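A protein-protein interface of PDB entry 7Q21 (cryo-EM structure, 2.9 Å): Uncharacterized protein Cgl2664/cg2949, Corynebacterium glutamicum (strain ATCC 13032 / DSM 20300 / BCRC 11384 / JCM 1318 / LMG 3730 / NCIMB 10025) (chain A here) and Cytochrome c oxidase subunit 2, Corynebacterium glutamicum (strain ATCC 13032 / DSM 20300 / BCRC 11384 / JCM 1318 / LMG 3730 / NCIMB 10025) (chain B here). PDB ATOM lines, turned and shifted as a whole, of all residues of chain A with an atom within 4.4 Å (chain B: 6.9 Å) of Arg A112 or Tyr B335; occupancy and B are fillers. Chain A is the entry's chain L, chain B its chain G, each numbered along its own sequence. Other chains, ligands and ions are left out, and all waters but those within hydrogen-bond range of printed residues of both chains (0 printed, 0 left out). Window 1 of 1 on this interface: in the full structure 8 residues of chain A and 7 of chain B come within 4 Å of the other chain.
O of Thr A85 is in hydrogen-bond range of OH of Tyr B335. The side-chain hydroxyl (OH) of Tyr B335 sits at hydrogen-bond distance from the guanidinium group (NH2) of Arg A112, 2.9 Å away.
The guanidinium group (NH1) of Arg B301 lies within hydrogen-bond range of the backbone carbonyl oxygen (O) of Tyr B335 (2.9 Å). O of Thr A85 lies close to ND1 of His A87. A ring nitrogen (NE2) of His A87 sits at hydrogen-bond distance from the guanidinium group of Arg A112, 3.3 Å away. SG of Cys A134 forms a disulfide with SG of Cys A114.
Thr B322 touches His A87. Ala B324 touches His A87 (CB to CE1, 3.6 Å). His A87 touches Gln B325. OE1 of Glu B328 touches CE1 of His A87, at 3.7 Å. CE1 of His A87 touches OH of Tyr B335, at 3.8 Å.
Of chain B, only Tyr B335 comes within 4 Å of Arg A112. Of chain A, only Thr A85 (2.5 Å), His A87 (3.8 Å) and Arg A112 (2.9 Å) come within 4 Å of Tyr B335. Of the printed residues of chain A, Glu B328 touches His A87. Of the printed residues of chain B, His A87 touches Thr B322, Ala B324, Gln B325, Glu B328 and Tyr B335. Printed residues of chain A within 4 Å of Gln B325: His A87. Of the printed residues of chain A, Ala B324 touches His A87 (3.6 Å). The nearest residue of chain B that does not touch Arg A112 is Ala B324 (4.1 Å). The nearest printed residue of chain B that does not touch His A87 is Pro B334 (5.3 Å).
Of the 10 printed residues of chain A, 3 touch a printed residue of chain B. Printed residues of chain A that touch a printed residue of chain B: Thr A85, His A87 and Arg A112. Hydrophobic or aromatic side chains of chain A that line the printed part of chain B: His A87. Hydrophobic or aromatic side chains of chain B within 4 Å of the printed part of chain A: Ala B324 and Tyr B335. Along chain B the printed residues that touch a printed residue of chain A span positions 322 to 335. Among the printed residues, 7 pairs touch across the chains.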
ATOM      1  N   ASN A  82      21.224 -14.105  14.299  1.00  0.00           N
ATOM      2  CA  ASN A  82      21.946 -14.194  13.042  1.00  0.00           C
ATOM      3  C   ASN A  82      23.000 -13.095  13.000  1.00  0.00           C
ATOM      4  O   ASN A  82      22.667 -11.919  12.807  1.00  0.00           O
ATOM      5  CB  ASN A  82      21.028 -14.122  11.824  1.00  0.00           C
ATOM      6  CG  ASN A  82      21.717 -14.482  10.523  1.00  0.00           C
ATOM      7  OD1 ASN A  82      22.668 -15.265  10.502  1.00  0.00           O
ATOM      8  ND2 ASN A  82      21.234 -13.930   9.426  1.00  0.00           N
ATOM      9  N   ASP A  84      25.924 -13.407  11.110  1.00  0.00           N
ATOM     10  CA  ASP A  84      26.804 -13.767  10.007  1.00  0.00           C
ATOM     11  C   ASP A  84      27.193 -12.510   9.237  1.00  0.00           C
ATOM     12  O   ASP A  84      26.328 -11.812   8.728  1.00  0.00           O
ATOM     13  CB  ASP A  84      26.176 -14.781   9.050  1.00  0.00           C
ATOM     14  CG  ASP A  84      27.170 -15.328   8.041  1.00  0.00           C
ATOM     15  OD1 ASP A  84      28.125 -16.011   8.462  1.00  0.00           O
ATOM     16  OD2 ASP A  84      27.014 -15.005   6.838  1.00  0.00           O
ATOM     17  N   THR A  85      28.507 -12.313   9.095  1.00  0.00           N
ATOM     18  CA  THR A  85      29.076 -11.123   8.486  1.00  0.00           C
ATOM     19  C   THR A  85      28.668 -11.003   7.019  1.00  0.00           C
ATOM     20  O   THR A  85      28.504  -9.894   6.524  1.00  0.00           O
ATOM     21  CB  THR A  85      30.599 -11.091   8.670  1.00  0.00           C
ATOM     22  OG1 THR A  85      31.149 -12.247   8.039  1.00  0.00           O
ATOM     23  CG2 THR A  85      31.016 -11.046  10.126  1.00  0.00           C
ATOM     24  N   HIS A  87      25.928 -11.131   4.868  1.00  0.00           N
ATOM     25  CA  HIS A  87      24.479 -11.057   5.019  1.00  0.00           C
ATOM     26  C   HIS A  87      23.789 -12.046   4.084  1.00  0.00           C
ATOM     27  O   HIS A  87      23.861 -11.891   2.865  1.00  0.00           O
ATOM     28  CB  HIS A  87      23.984  -9.629   4.782  1.00  0.00           C
ATOM     29  CG  HIS A  87      24.937  -8.600   5.280  1.00  0.00           C
ATOM     30  ND1 HIS A  87      26.095  -8.286   4.608  1.00  0.00           N
ATOM     31  CD2 HIS A  87      24.882  -7.774   6.348  1.00  0.00           C
ATOM     32  CE1 HIS A  87      26.729  -7.322   5.257  1.00  0.00           C
ATOM     33  NE2 HIS A  87      26.013  -7.007   6.338  1.00  0.00           N
ATOM     34  N   ILE A 110      15.826 -14.589   9.639  1.00  0.00           N
ATOM     35  CA  ILE A 110      16.652 -13.688  10.433  1.00  0.00           C
ATOM     36  C   ILE A 110      17.689 -13.054   9.505  1.00  0.00           C
ATOM     37  O   ILE A 110      18.564 -13.748   9.001  1.00  0.00           O
ATOM     38  CB  ILE A 110      17.294 -14.425  11.633  1.00  0.00           C
ATOM     39  CG1 ILE A 110      16.348 -15.444  12.276  1.00  0.00           C
ATOM     40  CG2 ILE A 110      17.792 -13.436  12.669  1.00  0.00           C
ATOM     41  CD1 ILE A 110      17.039 -16.441  13.187  1.00  0.00           C
ATOM     42  N   GLU A 111      17.585 -11.735   9.278  1.00  0.00           N
ATOM     43  CA  GLU A 111      18.354 -11.021   8.269  1.00  0.00           C
ATOM     44  C   GLU A 111      19.816 -10.826   8.680  1.00  0.00           C
ATOM     45  O   GLU A 111      20.732 -11.339   8.032  1.00  0.00           O
ATOM     46  CB  GLU A 111      17.676  -9.672   8.018  1.00  0.00           C
ATOM     47  CG  GLU A 111      16.447  -9.763   7.131  1.00  0.00           C
ATOM     48  CD  GLU A 111      16.651 -10.421   5.775  1.00  0.00           C
ATOM     49  OE1 GLU A 111      17.704 -10.183   5.138  1.00  0.00           O
ATOM     50  OE2 GLU A 111      15.743 -11.150   5.336  1.00  0.00           O
ATOM     51  N   ARG A 112      20.008  -9.991   9.708  1.00  0.00           N
ATOM     52  CA  ARG A 112      21.315  -9.688  10.277  1.00  0.00           C
ATOM     53  C   ARG A 112      21.120  -8.837  11.530  1.00  0.00           C
ATOM     54  O   ARG A 112      20.248  -7.964  11.558  1.00  0.00           O
ATOM     55  CB  ARG A 112      22.228  -8.991   9.259  1.00  0.00           C
ATOM     56  CG  ARG A 112      23.616  -9.609   9.158  1.00  0.00           C
ATOM     57  CD  ARG A 112      24.678  -9.063  10.097  1.00  0.00           C
ATOM     58  NE  ARG A 112      25.632  -8.191   9.430  1.00  0.00           N
ATOM     59  CZ  ARG A 112      26.756  -7.735   9.970  1.00  0.00           C
ATOM     60  NH1 ARG A 112      27.094  -8.065  11.206  1.00  0.00           N
ATOM     61  NH2 ARG A 112      27.545  -6.947   9.262  1.00  0.00           N
ATOM     62  N   ASN A 113      21.922  -9.129  12.567  1.00  0.00           N
ATOM     63  CA  ASN A 113      21.855  -8.469  13.860  1.00  0.00           C
ATOM     64  C   ASN A 113      20.418  -8.457  14.387  1.00  0.00           C
ATOM     65  O   ASN A 113      20.084  -7.607  15.195  1.00  0.00           O
ATOM     66  CB  ASN A 113      22.461  -7.060  13.818  1.00  0.00           C
ATOM     67  CG  ASN A 113      23.973  -7.036  13.809  1.00  0.00           C
ATOM     68  OD1 ASN A 113      24.635  -8.021  14.135  1.00  0.00           O
ATOM     69  ND2 ASN A 113      24.532  -5.888  13.464  1.00  0.00           N
ATOM     70  N   CYS A 114      19.575  -9.366  13.879  1.00  0.00           N
ATOM     71  CA  CYS A 114      18.202  -9.534  14.316  1.00  0.00           C
ATOM     72  C   CYS A 114      18.148 -10.615  15.398  1.00  0.00           C
ATOM     73  O   CYS A 114      19.202 -11.041  15.868  1.00  0.00           O
ATOM     74  CB  CYS A 114      17.333  -9.906  13.122  1.00  0.00           C
ATOM     75  SG  CYS A 114      16.871  -8.532  12.034  1.00  0.00           S
ATOM     76  N   CYS A 134      15.115  -5.306  15.439  1.00  0.00           N
ATOM     77  CA  CYS A 134      14.400  -6.314  14.674  1.00  0.00           C
ATOM     78  C   CYS A 134      14.388  -7.613  15.475  1.00  0.00           C
ATOM     79  O   CYS A 134      15.297  -8.430  15.354  1.00  0.00           O
ATOM     80  CB  CYS A 134      14.984  -6.488  13.273  1.00  0.00           C
ATOM     81  SG  CYS A 134      16.751  -6.896  13.239  1.00  0.00           S
ATOM     82  N   ASP B 220      33.281  -6.635  17.804  1.00  0.00           N
ATOM     83  CA  ASP B 220      33.701  -7.505  16.718  1.00  0.00           C
ATOM     84  C   ASP B 220      33.245  -6.943  15.373  1.00  0.00           C
ATOM     85  O   ASP B 220      32.983  -7.703  14.440  1.00  0.00           O
ATOM     86  CB  ASP B 220      33.206  -8.933  16.957  1.00  0.00           C
ATOM     87  CG  ASP B 220      31.714  -9.005  17.231  1.00  0.00           C
ATOM     88  OD1 ASP B 220      31.014  -8.002  16.966  1.00  0.00           O
ATOM     89  OD2 ASP B 220      31.266 -10.060  17.723  1.00  0.00           O
ATOM     90  N   GLU B 221      33.144  -5.612  15.290  1.00  0.00           N
ATOM     91  CA  GLU B 221      32.841  -4.910  14.051  1.00  0.00           C
ATOM     92  C   GLU B 221      33.306  -3.462  14.184  1.00  0.00           C
ATOM     93  O   GLU B 221      32.718  -2.688  14.937  1.00  0.00           O
ATOM     94  CB  GLU B 221      31.349  -5.032  13.731  1.00  0.00           C
ATOM     95  CG  GLU B 221      31.013  -4.815  12.268  1.00  0.00           C
ATOM     96  CD  GLU B 221      30.468  -3.438  11.925  1.00  0.00           C
ATOM     97  OE1 GLU B 221      29.987  -2.735  12.842  1.00  0.00           O
ATOM     98  OE2 GLU B 221      30.517  -3.069  10.734  1.00  0.00           O
ATOM     99  N   ILE B 222      34.379  -3.116  13.462  1.00  0.00           N
ATOM    100  CA  ILE B 222      34.992  -1.800  13.559  1.00  0.00           C
ATOM    101  C   ILE B 222      34.075  -0.769  12.903  1.00  0.00           C
ATOM    102  O   ILE B 222      33.717  -0.921  11.735  1.00  0.00           O
ATOM    103  CB  ILE B 222      36.412  -1.793  12.951  1.00  0.00           C
ATOM    104  CG1 ILE B 222      37.395  -2.664  13.744  1.00  0.00           C
ATOM    105  CG2 ILE B 222      36.928  -0.373  12.758  1.00  0.00           C
ATOM    106  CD1 ILE B 222      37.581  -2.279  15.200  1.00  0.00           C
ATOM    107  N   VAL B 224      32.864   2.222  10.808  1.00  0.00           N
ATOM    108  CA  VAL B 224      33.394   2.944   9.667  1.00  0.00           C
ATOM    109  C   VAL B 224      32.527   4.177   9.440  1.00  0.00           C
ATOM    110  O   VAL B 224      31.321   4.070   9.238  1.00  0.00           O
ATOM    111  CB  VAL B 224      33.475   2.053   8.413  1.00  0.00           C
ATOM    112  CG1 VAL B 224      33.740   2.859   7.151  1.00  0.00           C
ATOM    113  CG2 VAL B 224      34.514   0.956   8.571  1.00  0.00           C
ATOM    114  N   ALA B 280      40.916   4.559   3.039  1.00  0.00           N
ATOM    115  CA  ALA B 280      40.573   4.162   4.396  1.00  0.00           C
ATOM    116  C   ALA B 280      41.692   4.564   5.349  1.00  0.00           C
ATOM    117  O   ALA B 280      42.858   4.251   5.106  1.00  0.00           O
ATOM    118  CB  ALA B 280      40.316   2.678   4.444  1.00  0.00           C
ATOM    119  N   GLU B 299      37.445   3.597  11.733  1.00  0.00           N
ATOM    120  CA  GLU B 299      37.968   3.851  10.404  1.00  0.00           C
ATOM    121  C   GLU B 299      37.199   5.000   9.761  1.00  0.00           C
ATOM    122  O   GLU B 299      36.019   5.197  10.039  1.00  0.00           O
ATOM    123  CB  GLU B 299      37.902   2.591   9.543  1.00  0.00           C
ATOM    124  CG  GLU B 299      38.838   2.657   8.352  1.00  0.00           C
ATOM    125  CD  GLU B 299      38.537   1.679   7.234  1.00  0.00           C
ATOM    126  OE1 GLU B 299      37.612   1.951   6.440  1.00  0.00           O
ATOM    127  OE2 GLU B 299      39.240   0.656   7.151  1.00  0.00           O
ATOM    128  N   ARG B 301      36.256   6.151   5.934  1.00  0.00           N
ATOM    129  CA  ARG B 301      36.215   5.820   4.522  1.00  0.00           C
ATOM    130  C   ARG B 301      35.833   7.075   3.749  1.00  0.00           C
ATOM    131  O   ARG B 301      34.671   7.477   3.748  1.00  0.00           O
ATOM    132  CB  ARG B 301      35.233   4.677   4.256  1.00  0.00           C
ATOM    133  CG  ARG B 301      35.368   4.057   2.873  1.00  0.00           C
ATOM    134  CD  ARG B 301      36.570   3.138   2.754  1.00  0.00           C
ATOM    135  NE  ARG B 301      36.563   2.102   3.783  1.00  0.00           N
ATOM    136  CZ  ARG B 301      36.045   0.885   3.639  1.00  0.00           C
ATOM    137  NH1 ARG B 301      36.091   0.027   4.643  1.00  0.00           N
ATOM    138  NH2 ARG B 301      35.487   0.526   2.495  1.00  0.00           N
ATOM    139  N   ASP B 320      16.370  -0.080   7.928  1.00  0.00           N
ATOM    140  CA  ASP B 320      16.521  -1.404   8.507  1.00  0.00           C
ATOM    141  C   ASP B 320      17.821  -2.053   8.035  1.00  0.00           C
ATOM    142  O   ASP B 320      18.197  -3.112   8.538  1.00  0.00           O
ATOM    143  CB  ASP B 320      15.284  -2.264   8.230  1.00  0.00           C
ATOM    144  CG  ASP B 320      15.006  -3.305   9.303  1.00  0.00           C
ATOM    145  OD1 ASP B 320      15.686  -3.271  10.351  1.00  0.00           O
ATOM    146  OD2 ASP B 320      14.110  -4.144   9.081  1.00  0.00           O
ATOM    147  N   THR B 322      22.069  -2.262   7.156  1.00  0.00           N
ATOM    148  CA  THR B 322      23.270  -2.153   7.969  1.00  0.00           C
ATOM    149  C   THR B 322      24.346  -1.400   7.193  1.00  0.00           C
ATOM    150  O   THR B 322      24.302  -1.349   5.965  1.00  0.00           O
ATOM    151  CB  THR B 322      23.742  -3.527   8.464  1.00  0.00           C
ATOM    152  OG1 THR B 322      24.746  -3.282   9.449  1.00  0.00           O
ATOM    153  CG2 THR B 322      24.326  -4.393   7.368  1.00  0.00           C
ATOM    154  N   ASN B 323      25.328  -0.870   7.932  1.00  0.00           N
ATOM    155  CA  ASN B 323      26.386  -0.040   7.381  1.00  0.00           C
ATOM    156  C   ASN B 323      27.174  -0.796   6.314  1.00  0.00           C
ATOM    157  O   ASN B 323      27.543  -0.210   5.299  1.00  0.00           O
ATOM    158  CB  ASN B 323      27.304   0.516   8.470  1.00  0.00           C
ATOM    159  CG  ASN B 323      28.361   1.449   7.920  1.00  0.00           C
ATOM    160  OD1 ASN B 323      28.106   2.218   6.995  1.00  0.00           O
ATOM    161  ND2 ASN B 323      29.556   1.387   8.481  1.00  0.00           N
ATOM    162  N   ALA B 324      27.420  -2.090   6.556  1.00  0.00           N
ATOM    163  CA  ALA B 324      28.167  -2.929   5.631  1.00  0.00           C
ATOM    164  C   ALA B 324      27.419  -3.058   4.304  1.00  0.00           C
ATOM    165  O   ALA B 324      28.034  -2.972   3.245  1.00  0.00           O
ATOM    166  CB  ALA B 324      28.457  -4.270   6.256  1.00  0.00           C
ATOM    167  N   GLN B 325      26.092  -3.234   4.379  1.00  0.00           N
ATOM    168  CA  GLN B 325      25.249  -3.351   3.198  1.00  0.00           C
ATOM    169  C   GLN B 325      25.277  -2.050   2.396  1.00  0.00           C
ATOM    170  O   GLN B 325      25.362  -2.085   1.169  1.00  0.00           O
ATOM    171  CB  GLN B 325      23.830  -3.774   3.579  1.00  0.00           C
ATOM    172  CG  GLN B 325      23.634  -5.283   3.579  1.00  0.00           C
ATOM    173  CD  GLN B 325      22.290  -5.689   4.133  1.00  0.00           C
ATOM    174  OE1 GLN B 325      22.100  -5.791   5.343  1.00  0.00           O
ATOM    175  NE2 GLN B 325      21.345  -5.939   3.242  1.00  0.00           N
ATOM    176  N   LEU B 327      27.707   0.166   2.422  1.00  0.00           N
ATOM    177  CA  LEU B 327      29.041   0.267   1.848  1.00  0.00           C
ATOM    178  C   LEU B 327      29.136  -0.588   0.587  1.00  0.00           C
ATOM    179  O   LEU B 327      29.720  -0.148  -0.399  1.00  0.00           O
ATOM    180  CB  LEU B 327      30.098  -0.136   2.883  1.00  0.00           C
ATOM    181  CG  LEU B 327      30.582   0.977   3.814  1.00  0.00           C
ATOM    182  CD1 LEU B 327      31.246   0.390   5.048  1.00  0.00           C
ATOM    183  CD2 LEU B 327      31.539   1.922   3.099  1.00  0.00           C
ATOM    184  N   GLU B 328      28.543  -1.790   0.624  1.00  0.00           N
ATOM    185  CA  GLU B 328      28.509  -2.687  -0.522  1.00  0.00           C
ATOM    186  C   GLU B 328      27.707  -2.060  -1.663  1.00  0.00           C
ATOM    187  O   GLU B 328      27.997  -2.323  -2.829  1.00  0.00           O
ATOM    188  CB  GLU B 328      27.911  -4.048  -0.157  1.00  0.00           C
ATOM    189  CG  GLU B 328      28.816  -4.924   0.695  1.00  0.00           C
ATOM    190  CD  GLU B 328      28.150  -6.158   1.286  1.00  0.00           C
ATOM    191  OE1 GLU B 328      28.727  -6.748   2.218  1.00  0.00           O
ATOM    192  OE2 GLU B 328      27.059  -6.539   0.807  1.00  0.00           O
ATOM    193  N   GLN B 332      32.083  -0.311  -2.193  1.00  0.00           N
ATOM    194  CA  GLN B 332      33.173  -0.245  -1.232  1.00  0.00           C
ATOM    195  C   GLN B 332      33.324  -1.592  -0.529  1.00  0.00           C
ATOM    196  O   GLN B 332      32.435  -2.442  -0.596  1.00  0.00           O
ATOM    197  CB  GLN B 332      32.923   0.875  -0.218  1.00  0.00           C
ATOM    198  CG  GLN B 332      32.962   2.277  -0.811  1.00  0.00           C
ATOM    199  CD  GLN B 332      34.340   2.698  -1.260  1.00  0.00           C
ATOM    200  OE1 GLN B 332      35.347   2.398  -0.620  1.00  0.00           O
ATOM    201  NE2 GLN B 332      34.391   3.408  -2.375  1.00  0.00           N
ATOM    202  N   ALA B 333      34.467  -1.775   0.144  1.00  0.00           N
ATOM    203  CA  ALA B 333      34.670  -2.912   1.027  1.00  0.00           C
ATOM    204  C   ALA B 333      33.737  -2.777   2.229  1.00  0.00           C
ATOM    205  O   ALA B 333      33.675  -1.715   2.847  1.00  0.00           O
ATOM    206  CB  ALA B 333      36.117  -2.997   1.443  1.00  0.00           C
ATOM    207  N   PRO B 334      32.973  -3.833   2.595  1.00  0.00           N
ATOM    208  CA  PRO B 334      31.976  -3.723   3.660  1.00  0.00           C
ATOM    209  C   PRO B 334      32.557  -3.509   5.058  1.00  0.00           C
ATOM    210  O   PRO B 334      31.864  -3.003   5.938  1.00  0.00           O
ATOM    211  CB  PRO B 334      31.217  -5.053   3.585  1.00  0.00           C
ATOM    212  CG  PRO B 334      32.226  -6.014   3.000  1.00  0.00           C
ATOM    213  CD  PRO B 334      33.026  -5.185   2.017  1.00  0.00           C
ATOM    214  N   TYR B 335      33.830  -3.879   5.244  1.00  0.00           N
ATOM    215  CA  TYR B 335      34.453  -3.826   6.558  1.00  0.00           C
ATOM    216  C   TYR B 335      35.758  -3.036   6.509  1.00  0.00           C
ATOM    217  O   TYR B 335      36.293  -2.771   5.433  1.00  0.00           O
ATOM    218  CB  TYR B 335      34.598  -5.235   7.140  1.00  0.00           C
ATOM    219  CG  TYR B 335      33.290  -5.974   7.272  1.00  0.00           C
ATOM    220  CD1 TYR B 335      32.379  -5.635   8.261  1.00  0.00           C
ATOM    221  CD2 TYR B 335      32.951  -6.995   6.396  1.00  0.00           C
ATOM    222  CE1 TYR B 335      31.166  -6.296   8.383  1.00  0.00           C
ATOM    223  CE2 TYR B 335      31.740  -7.665   6.501  1.00  0.00           C
ATOM    224  CZ  TYR B 335      30.849  -7.315   7.503  1.00  0.00           C
ATOM    225  OH  TYR B 335      29.655  -7.959   7.630  1.00  0.00           O
ATOM    226  N   ALA B 336      36.249  -2.665   7.700  1.00  0.00           N
ATOM    227  CA  ALA B 336      37.465  -1.882   7.859  1.00  0.00           C
ATOM    228  C   ALA B 336      38.658  -2.627   7.267  1.00  0.00           C
ATOM    229  O   ALA B 336      38.849  -3.814   7.523  1.00  0.00           O
ATOM    230  CB  ALA B 336      37.685  -1.548   9.314  1.00  0.00           C
ATOM    231  N   THR B 337      39.452  -1.899   6.476  1.00  0.00           N
ATOM    232  CA  THR B 337      40.592  -2.468   5.773  1.00  0.00           C
ATOM    233  C   THR B 337      41.901  -2.091   6.466  1.00  0.00           C
ATOM    234  O   THR B 337      42.874  -2.839   6.386  1.00  0.00           O
ATOM    235  CB  THR B 337      40.589  -2.071   4.292  1.00  0.00           C
ATOM    236  OG1 THR B 337      40.781  -0.658   4.215  1.00  0.00           O
ATOM    237  CG2 THR B 337      39.313  -2.461   3.576  1.00  0.00           C
ATOM    238  N   SER B 338      41.917  -0.928   7.130  1.00  0.00           N
ATOM    239  CA  SER B 338      43.106  -0.421   7.803  1.00  0.00           C
ATOM    240  C   SER B 338      43.182  -0.914   9.249  1.00  0.00           C
ATOM    241  O   SER B 338      44.197  -0.722   9.917  1.00  0.00           O
ATOM    242  CB  SER B 338      43.156   1.081   7.730  1.00  0.00           C
ATOM    243  OG  SER B 338      41.941   1.638   8.206  1.00  0.00           O
ATOM    244  N   THR B 339      42.098  -1.538   9.727  1.00  0.00           N
ATOM    245  CA  THR B 339      42.011  -2.036  11.091  1.00  0.00           C
ATOM    246  C   THR B 339      41.225  -3.343  11.093  1.00  0.00           C
ATOM    247  O   THR B 339      40.396  -3.573  10.216  1.00  0.00           O
ATOM    248  CB  THR B 339      41.355  -1.003  12.020  1.00  0.00           C
ATOM    249  OG1 THR B 339      41.943   0.276  11.796  1.00  0.00           O
ATOM    250  CG2 THR B 339      41.483  -1.347  13.488  1.00  0.00           C
